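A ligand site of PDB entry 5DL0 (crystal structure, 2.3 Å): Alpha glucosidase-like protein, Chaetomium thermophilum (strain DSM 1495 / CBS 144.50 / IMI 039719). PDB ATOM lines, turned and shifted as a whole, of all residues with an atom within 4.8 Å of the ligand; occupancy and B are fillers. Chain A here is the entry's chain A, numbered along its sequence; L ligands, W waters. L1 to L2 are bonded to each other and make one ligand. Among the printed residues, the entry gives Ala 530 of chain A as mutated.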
ATOM      1  N   HIS A   8      28.565 -10.176  11.753  1.00  0.00           N
ATOM      2  CA  HIS A   8      29.184 -11.143  12.646  1.00  0.00           C
ATOM      3  C   HIS A   8      29.942 -12.140  11.756  1.00  0.00           C
ATOM      4  O   HIS A   8      29.416 -12.618  10.759  1.00  0.00           O
ATOM      5  CB  HIS A   8      28.109 -11.817  13.521  1.00  0.00           C
ATOM      6  CG  HIS A   8      27.531 -10.911  14.578  1.00  0.00           C
ATOM      7  ND1 HIS A   8      26.928  -9.699  14.282  1.00  0.00           N
ATOM      8  CD2 HIS A   8      27.460 -11.034  15.930  1.00  0.00           C
ATOM      9  CE1 HIS A   8      26.517  -9.124  15.394  1.00  0.00           C
ATOM     10  NE2 HIS A   8      26.826  -9.917  16.408  1.00  0.00           N
ATOM     11  N   ASP A 277      27.964 -16.277  21.127  1.00  0.00           N
ATOM     12  CA  ASP A 277      26.826 -15.395  21.089  1.00  0.00           C
ATOM     13  C   ASP A 277      26.484 -15.157  19.629  1.00  0.00           C
ATOM     14  O   ASP A 277      27.081 -14.287  19.007  1.00  0.00           O
ATOM     15  CB  ASP A 277      27.172 -14.072  21.786  1.00  0.00           C
ATOM     16  CG  ASP A 277      25.965 -13.139  21.913  1.00  0.00           C
ATOM     17  OD1 ASP A 277      24.891 -13.377  21.275  1.00  0.00           O
ATOM     18  OD2 ASP A 277      26.111 -12.150  22.686  1.00  0.00           O
ATOM     19  N   PHE A 279      24.133 -13.870  17.101  1.00  0.00           N
ATOM     20  CA  PHE A 279      23.056 -12.948  16.791  1.00  0.00           C
ATOM     21  C   PHE A 279      22.288 -13.389  15.547  1.00  0.00           C
ATOM     22  O   PHE A 279      22.866 -13.596  14.500  1.00  0.00           O
ATOM     23  CB  PHE A 279      23.716 -11.569  16.579  1.00  0.00           C
ATOM     24  CG  PHE A 279      22.768 -10.459  16.170  1.00  0.00           C
ATOM     25  CD1 PHE A 279      21.872  -9.931  17.069  1.00  0.00           C
ATOM     26  CD2 PHE A 279      22.847  -9.903  14.888  1.00  0.00           C
ATOM     27  CE1 PHE A 279      21.042  -8.872  16.702  1.00  0.00           C
ATOM     28  CE2 PHE A 279      22.017  -8.861  14.510  1.00  0.00           C
ATOM     29  CZ  PHE A 279      21.122  -8.341  15.419  1.00  0.00           C
ATOM     30  N   TRP A 389      12.778  -7.430  27.057  1.00  0.00           N
ATOM     31  CA  TRP A 389      13.797  -6.402  27.154  1.00  0.00           C
ATOM     32  C   TRP A 389      13.102  -5.095  26.758  1.00  0.00           C
ATOM     33  O   TRP A 389      12.935  -4.819  25.560  1.00  0.00           O
ATOM     34  CB  TRP A 389      14.946  -6.781  26.216  1.00  0.00           C
ATOM     35  CG  TRP A 389      16.160  -5.868  26.225  1.00  0.00           C
ATOM     36  CD1 TRP A 389      16.468  -4.923  27.165  1.00  0.00           C
ATOM     37  CD2 TRP A 389      17.216  -5.843  25.254  1.00  0.00           C
ATOM     38  NE1 TRP A 389      17.646  -4.309  26.836  1.00  0.00           N
ATOM     39  CE2 TRP A 389      18.131  -4.842  25.671  1.00  0.00           C
ATOM     40  CE3 TRP A 389      17.484  -6.543  24.088  1.00  0.00           C
ATOM     41  CZ2 TRP A 389      19.292  -4.529  24.939  1.00  0.00           C
ATOM     42  CZ3 TRP A 389      18.652  -6.234  23.361  1.00  0.00           C
ATOM     43  CH2 TRP A 389      19.532  -5.238  23.784  1.00  0.00           C
ATOM     44  N   ASP A 417      15.150  -7.673  32.667  1.00  0.00           N
ATOM     45  CA  ASP A 417      16.358  -7.598  31.873  1.00  0.00           C
ATOM     46  C   ASP A 417      17.230  -6.353  32.242  1.00  0.00           C
ATOM     47  O   ASP A 417      16.895  -5.579  33.134  1.00  0.00           O
ATOM     48  CB  ASP A 417      15.941  -7.576  30.382  1.00  0.00           C
ATOM     49  CG  ASP A 417      16.905  -8.321  29.479  1.00  0.00           C
ATOM     50  OD1 ASP A 417      18.138  -8.220  29.666  1.00  0.00           O
ATOM     51  OD2 ASP A 417      16.404  -8.978  28.525  1.00  0.00           O
ATOM     52  N   ILE A 418      18.320  -6.170  31.498  1.00  0.00           N
ATOM     53  CA  ILE A 418      19.488  -5.385  31.934  1.00  0.00           C
ATOM     54  C   ILE A 418      19.234  -3.898  32.245  1.00  0.00           C
ATOM     55  O   ILE A 418      20.004  -3.307  33.047  1.00  0.00           O
ATOM     56  CB  ILE A 418      20.654  -5.455  30.913  1.00  0.00           C
ATOM     57  CG1 ILE A 418      20.207  -5.076  29.493  1.00  0.00           C
ATOM     58  CG2 ILE A 418      21.279  -6.830  30.940  1.00  0.00           C
ATOM     59  CD1 ILE A 418      21.359  -5.123  28.490  1.00  0.00           C
ATOM     60  N   ILE A 454      18.312 -10.311  35.841  1.00  0.00           N
ATOM     61  CA  ILE A 454      19.532 -10.694  35.150  1.00  0.00           C
ATOM     62  C   ILE A 454      20.844 -10.229  35.860  1.00  0.00           C
ATOM     63  O   ILE A 454      20.946  -9.090  36.324  1.00  0.00           O
ATOM     64  CB  ILE A 454      19.454 -10.226  33.674  1.00  0.00           C
ATOM     65  CG1 ILE A 454      20.563 -10.871  32.843  1.00  0.00           C
ATOM     66  CG2 ILE A 454      19.522  -8.728  33.561  1.00  0.00           C
ATOM     67  CD1 ILE A 454      20.244 -10.803  31.345  1.00  0.00           C
ATOM     68  N   TRP A 491      27.831  -4.868  27.583  1.00  0.00           N
ATOM     69  CA  TRP A 491      26.801  -3.851  27.874  1.00  0.00           C
ATOM     70  C   TRP A 491      27.363  -2.598  28.558  1.00  0.00           C
ATOM     71  O   TRP A 491      27.025  -1.505  28.132  1.00  0.00           O
ATOM     72  CB  TRP A 491      25.634  -4.423  28.689  1.00  0.00           C
ATOM     73  CG  TRP A 491      24.898  -5.595  28.022  1.00  0.00           C
ATOM     74  CD1 TRP A 491      24.736  -6.830  28.535  1.00  0.00           C
ATOM     75  CD2 TRP A 491      24.283  -5.599  26.728  1.00  0.00           C
ATOM     76  NE1 TRP A 491      24.038  -7.617  27.648  1.00  0.00           N
ATOM     77  CE2 TRP A 491      23.743  -6.887  26.534  1.00  0.00           C
ATOM     78  CE3 TRP A 491      24.093  -4.636  25.742  1.00  0.00           C
ATOM     79  CZ2 TRP A 491      23.044  -7.244  25.381  1.00  0.00           C
ATOM     80  CZ3 TRP A 491      23.394  -4.994  24.589  1.00  0.00           C
ATOM     81  CH2 TRP A 491      22.884  -6.281  24.429  1.00  0.00           C
ATOM     82  N   TRP A 528      18.836 -14.888  36.432  1.00  0.00           N
ATOM     83  CA  TRP A 528      19.029 -15.233  35.047  1.00  0.00           C
ATOM     84  C   TRP A 528      20.481 -14.862  34.706  1.00  0.00           C
ATOM     85  O   TRP A 528      20.895 -13.724  34.931  1.00  0.00           O
ATOM     86  CB  TRP A 528      18.034 -14.344  34.261  1.00  0.00           C
ATOM     87  CG  TRP A 528      18.151 -14.331  32.808  1.00  0.00           C
ATOM     88  CD1 TRP A 528      18.780 -15.239  32.044  1.00  0.00           C
ATOM     89  CD2 TRP A 528      17.561 -13.395  31.925  1.00  0.00           C
ATOM     90  NE1 TRP A 528      18.657 -14.914  30.712  1.00  0.00           N
ATOM     91  CE2 TRP A 528      17.914 -13.774  30.610  1.00  0.00           C
ATOM     92  CE3 TRP A 528      16.812 -12.251  32.106  1.00  0.00           C
ATOM     93  CZ2 TRP A 528      17.508 -13.074  29.499  1.00  0.00           C
ATOM     94  CZ3 TRP A 528      16.419 -11.526  30.978  1.00  0.00           C
ATOM     95  CH2 TRP A 528      16.768 -11.958  29.685  1.00  0.00           C
ATOM     96  N   ALA A 530      23.013 -14.668  31.486  1.00  0.00           N
ATOM     97  CA  ALA A 530      23.273 -14.689  30.034  1.00  0.00           C
ATOM     98  C   ALA A 530      24.684 -14.170  29.761  1.00  0.00           C
ATOM     99  O   ALA A 530      25.407 -13.833  30.704  1.00  0.00           O
ATOM    100  CB  ALA A 530      22.259 -13.806  29.324  1.00  0.00           C
ATOM    101  N   MET A 531      25.072 -14.114  28.480  1.00  0.00           N
ATOM    102  CA  MET A 531      26.355 -13.538  28.054  1.00  0.00           C
ATOM    103  C   MET A 531      27.536 -14.291  28.647  1.00  0.00           C
ATOM    104  O   MET A 531      28.678 -13.802  28.588  1.00  0.00           O
ATOM    105  CB  MET A 531      26.472 -12.057  28.425  1.00  0.00           C
ATOM    106  CG  MET A 531      25.198 -11.233  28.240  1.00  0.00           C
ATOM    107  SD  MET A 531      24.636 -11.232  26.534  1.00  0.00           S
ATOM    108  CE  MET A 531      25.729 -10.043  25.753  1.00  0.00           C
ATOM    109  N   SER A 535      30.283 -13.739  26.217  1.00  0.00           N
ATOM    110  CA  SER A 535      30.064 -12.809  25.139  1.00  0.00           C
ATOM    111  C   SER A 535      30.949 -11.594  25.363  1.00  0.00           C
ATOM    112  O   SER A 535      30.783 -10.890  26.359  1.00  0.00           O
ATOM    113  CB  SER A 535      28.597 -12.418  25.063  1.00  0.00           C
ATOM    114  OG  SER A 535      28.357 -11.454  24.073  1.00  0.00           O
ATOM    115  N   PHE A 537      31.905  -8.191  22.988  1.00  0.00           N
ATOM    116  CA  PHE A 537      31.414  -7.552  21.769  1.00  0.00           C
ATOM    117  C   PHE A 537      32.549  -7.265  20.800  1.00  0.00           C
ATOM    118  O   PHE A 537      32.412  -7.409  19.600  1.00  0.00           O
ATOM    119  CB  PHE A 537      30.654  -6.259  22.102  1.00  0.00           C
ATOM    120  CG  PHE A 537      29.302  -6.474  22.743  1.00  0.00           C
ATOM    121  CD1 PHE A 537      28.756  -7.752  22.907  1.00  0.00           C
ATOM    122  CD2 PHE A 537      28.555  -5.387  23.189  1.00  0.00           C
ATOM    123  CE1 PHE A 537      27.506  -7.924  23.493  1.00  0.00           C
ATOM    124  CE2 PHE A 537      27.312  -5.555  23.769  1.00  0.00           C
ATOM    125  CZ  PHE A 537      26.780  -6.832  23.916  1.00  0.00           C
ATOM    126  N   ARG A 591      22.244 -19.101  29.549  1.00  0.00           N
ATOM    127  CA  ARG A 591      22.373 -19.190  28.100  1.00  0.00           C
ATOM    128  C   ARG A 591      23.420 -20.209  27.659  1.00  0.00           C
ATOM    129  O   ARG A 591      23.118 -21.070  26.858  1.00  0.00           O
ATOM    130  CB  ARG A 591      22.649 -17.870  27.476  1.00  0.00           C
ATOM    131  CG  ARG A 591      22.247 -17.856  25.997  1.00  0.00           C
ATOM    132  CD  ARG A 591      22.201 -16.419  25.470  1.00  0.00           C
ATOM    133  NE  ARG A 591      23.531 -15.899  25.360  1.00  0.00           N
ATOM    134  CZ  ARG A 591      23.881 -14.704  24.877  1.00  0.00           C
ATOM    135  NH1 ARG A 591      25.158 -14.379  24.794  1.00  0.00           N
ATOM    136  NH2 ARG A 591      22.982 -13.864  24.417  1.00  0.00           N
ATOM    137  N   TRP A 604      17.659 -21.842  27.805  1.00  0.00           N
ATOM    138  CA  TRP A 604      16.816 -21.602  26.676  1.00  0.00           C
ATOM    139  C   TRP A 604      17.682 -21.449  25.470  1.00  0.00           C
ATOM    140  O   TRP A 604      18.888 -21.278  25.596  1.00  0.00           O
ATOM    141  CB  TRP A 604      15.936 -20.376  26.908  1.00  0.00           C
ATOM    142  CG  TRP A 604      16.471 -19.045  26.468  1.00  0.00           C
ATOM    143  CD1 TRP A 604      16.015 -18.280  25.451  1.00  0.00           C
ATOM    144  CD2 TRP A 604      17.525 -18.289  27.091  1.00  0.00           C
ATOM    145  NE1 TRP A 604      16.738 -17.117  25.350  1.00  0.00           N
ATOM    146  CE2 TRP A 604      17.655 -17.085  26.365  1.00  0.00           C
ATOM    147  CE3 TRP A 604      18.359 -18.508  28.174  1.00  0.00           C
ATOM    148  CZ2 TRP A 604      18.599 -16.130  26.693  1.00  0.00           C
ATOM    149  CZ3 TRP A 604      19.267 -17.551  28.515  1.00  0.00           C
ATOM    150  CH2 TRP A 604      19.391 -16.367  27.766  1.00  0.00           C
ATOM    151  N   ASP A 607      18.654 -16.323  21.196  1.00  0.00           N
ATOM    152  CA  ASP A 607      17.971 -15.308  20.420  1.00  0.00           C
ATOM    153  C   ASP A 607      17.351 -15.888  19.135  1.00  0.00           C
ATOM    154  O   ASP A 607      17.868 -15.755  18.060  1.00  0.00           O
ATOM    155  CB  ASP A 607      18.886 -14.116  20.152  1.00  0.00           C
ATOM    156  CG  ASP A 607      19.449 -13.514  21.439  1.00  0.00           C
ATOM    157  OD1 ASP A 607      18.789 -13.630  22.501  1.00  0.00           O
ATOM    158  OD2 ASP A 607      20.544 -12.945  21.389  1.00  0.00           O
ATOM    159  N   PHE A 640      12.279 -14.159  19.865  1.00  0.00           N
ATOM    160  CA  PHE A 640      12.914 -12.991  20.465  1.00  0.00           C
ATOM    161  C   PHE A 640      12.953 -11.788  19.499  1.00  0.00           C
ATOM    162  O   PHE A 640      12.413 -10.758  19.846  1.00  0.00           O
ATOM    163  CB  PHE A 640      14.319 -13.358  20.895  1.00  0.00           C
ATOM    164  CG  PHE A 640      15.105 -12.227  21.502  1.00  0.00           C
ATOM    165  CD1 PHE A 640      14.771 -11.700  22.749  1.00  0.00           C
ATOM    166  CD2 PHE A 640      16.270 -11.789  20.887  1.00  0.00           C
ATOM    167  CE1 PHE A 640      15.563 -10.707  23.324  1.00  0.00           C
ATOM    168  CE2 PHE A 640      17.069 -10.792  21.474  1.00  0.00           C
ATOM    169  CZ  PHE A 640      16.721 -10.281  22.692  1.00  0.00           C
ATOM    170  N   PHE A 641      13.595 -11.925  18.341  1.00  0.00           N
ATOM    171  CA  PHE A 641      13.661 -10.831  17.356  1.00  0.00           C
ATOM    172  C   PHE A 641      12.384 -10.663  16.544  1.00  0.00           C
ATOM    173  O   PHE A 641      11.876 -11.650  16.024  1.00  0.00           O
ATOM    174  CB  PHE A 641      14.757 -11.064  16.317  1.00  0.00           C
ATOM    175  CG  PHE A 641      16.131 -11.051  16.869  1.00  0.00           C
ATOM    176  CD1 PHE A 641      16.704  -9.851  17.321  1.00  0.00           C
ATOM    177  CD2 PHE A 641      16.868 -12.220  16.959  1.00  0.00           C
ATOM    178  CE1 PHE A 641      18.000  -9.837  17.852  1.00  0.00           C
ATOM    179  CE2 PHE A 641      18.170 -12.218  17.473  1.00  0.00           C
ATOM    180  CZ  PHE A 641      18.737 -11.030  17.925  1.00  0.00           C
ATOM    181  N   ARG A 663       8.808 -19.646  28.777  1.00  0.00           N
ATOM    182  CA  ARG A 663       8.943 -18.223  28.938  1.00  0.00           C
ATOM    183  C   ARG A 663       8.665 -17.485  27.645  1.00  0.00           C
ATOM    184  O   ARG A 663       9.109 -17.854  26.559  1.00  0.00           O
ATOM    185  CB  ARG A 663      10.356 -17.888  29.459  1.00  0.00           C
ATOM    186  CG  ARG A 663      10.665 -16.402  29.610  1.00  0.00           C
ATOM    187  CD  ARG A 663      12.108 -16.154  30.013  1.00  0.00           C
ATOM    188  NE  ARG A 663      13.057 -16.320  28.893  1.00  0.00           N
ATOM    189  CZ  ARG A 663      14.226 -15.694  28.766  1.00  0.00           C
ATOM    190  NH1 ARG A 663      14.667 -14.856  29.707  1.00  0.00           N
ATOM    191  NH2 ARG A 663      14.982 -15.936  27.708  1.00  0.00           N
ATOM    192  N   HIS A 665       9.442 -13.912  25.774  1.00  0.00           N
ATOM    193  CA  HIS A 665      10.547 -12.936  25.844  1.00  0.00           C
ATOM    194  C   HIS A 665      10.566 -12.207  24.508  1.00  0.00           C
ATOM    195  O   HIS A 665      10.042 -12.717  23.522  1.00  0.00           O
ATOM    196  CB  HIS A 665      11.903 -13.635  26.184  1.00  0.00           C
ATOM    197  CG  HIS A 665      13.049 -12.696  26.374  1.00  0.00           C
ATOM    198  ND1 HIS A 665      12.898 -11.428  26.905  1.00  0.00           N
ATOM    199  CD2 HIS A 665      14.373 -12.831  26.094  1.00  0.00           C
ATOM    200  CE1 HIS A 665      14.071 -10.820  26.922  1.00  0.00           C
ATOM    201  NE2 HIS A 665      14.987 -11.652  26.440  1.00  0.00           N
ATOM    202  N   HIS A 667      12.782  -8.939  22.120  1.00  0.00           N
ATOM    203  CA  HIS A 667      13.898  -8.031  21.895  1.00  0.00           C
ATOM    204  C   HIS A 667      13.436  -6.558  22.078  1.00  0.00           C
ATOM    205  O   HIS A 667      12.225  -6.273  22.110  1.00  0.00           O
ATOM    206  CB  HIS A 667      14.456  -8.308  20.501  1.00  0.00           C
ATOM    207  CG  HIS A 667      15.490  -7.343  20.007  1.00  0.00           C
ATOM    208  ND1 HIS A 667      16.850  -7.529  20.186  1.00  0.00           N
ATOM    209  CD2 HIS A 667      15.369  -6.233  19.246  1.00  0.00           C
ATOM    210  CE1 HIS A 667      17.521  -6.561  19.604  1.00  0.00           C
ATOM    211  NE2 HIS A 667      16.649  -5.743  19.039  1.00  0.00           N
HETATM  212  C1  LIG L   1      21.448  -8.453  20.775  1.00  0.00           C
HETATM  213  C2  LIG L   1      20.764  -9.343  21.809  1.00  0.00           C
HETATM  214  C3  LIG L   1      21.654  -9.972  22.897  1.00  0.00           C
HETATM  215  C4  LIG L   1      22.966 -10.458  22.265  1.00  0.00           C
HETATM  216  C5  LIG L   1      23.643  -9.343  21.430  1.00  0.00           C
HETATM  217  C6  LIG L   1      24.950  -9.763  20.724  1.00  0.00           C
HETATM  218  O1  LIG L   1      21.531  -7.123  21.213  1.00  0.00           O
HETATM  219  O2  LIG L   1      20.168 -10.388  21.060  1.00  0.00           O
HETATM  220  O3  LIG L   1      20.889 -10.812  23.639  1.00  0.00           O
HETATM  221  O4  LIG L   1      23.852 -10.918  23.239  1.00  0.00           O
HETATM  222  O5  LIG L   1      22.772  -8.898  20.426  1.00  0.00           O
HETATM  223  O6  LIG L   1      24.763 -10.930  19.939  1.00  0.00           O
HETATM  224  C1  LG2 L   2      21.104 -11.113  25.010  1.00  0.00           C
HETATM  225  C2  LG2 L   2      20.177 -12.212  25.539  1.00  0.00           C
HETATM  226  C3  LG2 L   2      18.709 -11.772  25.534  1.00  0.00           C
HETATM  227  C4  LG2 L   2      18.622 -10.490  26.386  1.00  0.00           C
HETATM  228  C5  LG2 L   2      19.639  -9.437  25.940  1.00  0.00           C
HETATM  229  C6  LG2 L   2      19.671  -8.223  26.875  1.00  0.00           C
HETATM  230  O1  LG2 L   2      20.340 -13.390  24.819  1.00  0.00           O
HETATM  231  O2  LG2 L   2      17.869 -12.813  26.021  1.00  0.00           O
HETATM  232  O3  LG2 L   2      17.308  -9.907  26.309  1.00  0.00           O
HETATM  233  O4  LG2 L   2      20.956  -9.918  25.776  1.00  0.00           O
HETATM  234  O5  LG2 L   2      20.170  -8.581  28.133  1.00  0.00           O
HETATM  235  O   HOH W   1      16.737 -14.481  24.117  1.00  0.00           O
HETATM  236  O   HOH W   2      22.418  -9.847  28.694  1.00  0.00           O
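Phe 279 touches the ligand.
Trp 389 touches the ligand.
CG2 of Ile 418 touches O5 of LG2 L2, 3.5 Å away.
Ile 454 touches the ligand.
Trp 491 touches the ligand.
CZ2 of Trp 528 touches O2 of LG2 L2, at 3.5 Å.
CZ2 of Trp 604 touches O2 of LG2 L2, 3.5 Å away.
CE2 of Phe 640 touches O2 of LIG L1, at 3.2 Å.
Phe 641 touches the ligand.
Hydrophobic or aromatic side chains that line the ligand: Phe 279, Trp 389, Ile 418, Ile 454, Trp 491, Trp 528, Met 531, Trp 604, Phe 640, Phe 641 and His 665.
Along chain A the residues within 4 Å of the ligand span positions 277 to 665.
NH1 of Arg 591 is in salt-bridge range of OD2 of Asp 277 (3.2 Å).
The side-chain carboxylate (OD2) of Asp 607 lies within salt-bridge range of the guanidinium group (NH2) of Arg 591.
The backbone carbonyl oxygen (O) of Phe 640 lies within hydrogen-bond range of the backbone NH (N) of His 667 (2.9 Å).
OD2 of Asp 277 lies within hydrogen-bond range of OG of Ser 535 (2.7 Å).
The side-chain sulfur (SD) of Met 531 lies close to the guanidinium group (NH1) of Arg 591, at 3.6 Å.
OD2 of Asp 417 lies within hydrogen-bond range of O3 of LG2 L2 (2.6 Å).
NE2 of His 665 sits at hydrogen-bond distance from O3 of LG2 L2 (2.9 Å).
An oxygen (O1) of LG2 L2 sits at hydrogen-bond distance from the guanidinium group (NH2) of Arg 591.
The side-chain sulfur (SD) of Met 531 sits close to an oxygen (O4) of LIG L1.
The side-chain carboxylate (OD2) of Asp 277 is in hydrogen-bond range of an oxygen (O4) of LIG L1 (2.6 Å).
An oxygen (O2) of LIG L1 lies within hydrogen-bond range of the side-chain carboxylate (OD2) of Asp 607, at 2.6 Å.
Water W2 lies within hydrogen-bond range of O5 of LG2 L2 (2.6 Å), NE1 of Trp 491 (2.9 Å) and SD of Met 531 (3.4 Å).
Water W1 lies within hydrogen-bond range of OD1 of Asp 607 (2.7 Å), O2 of LG2 L2 (2.8 Å) and NE1 of Trp 604 (2.9 Å).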
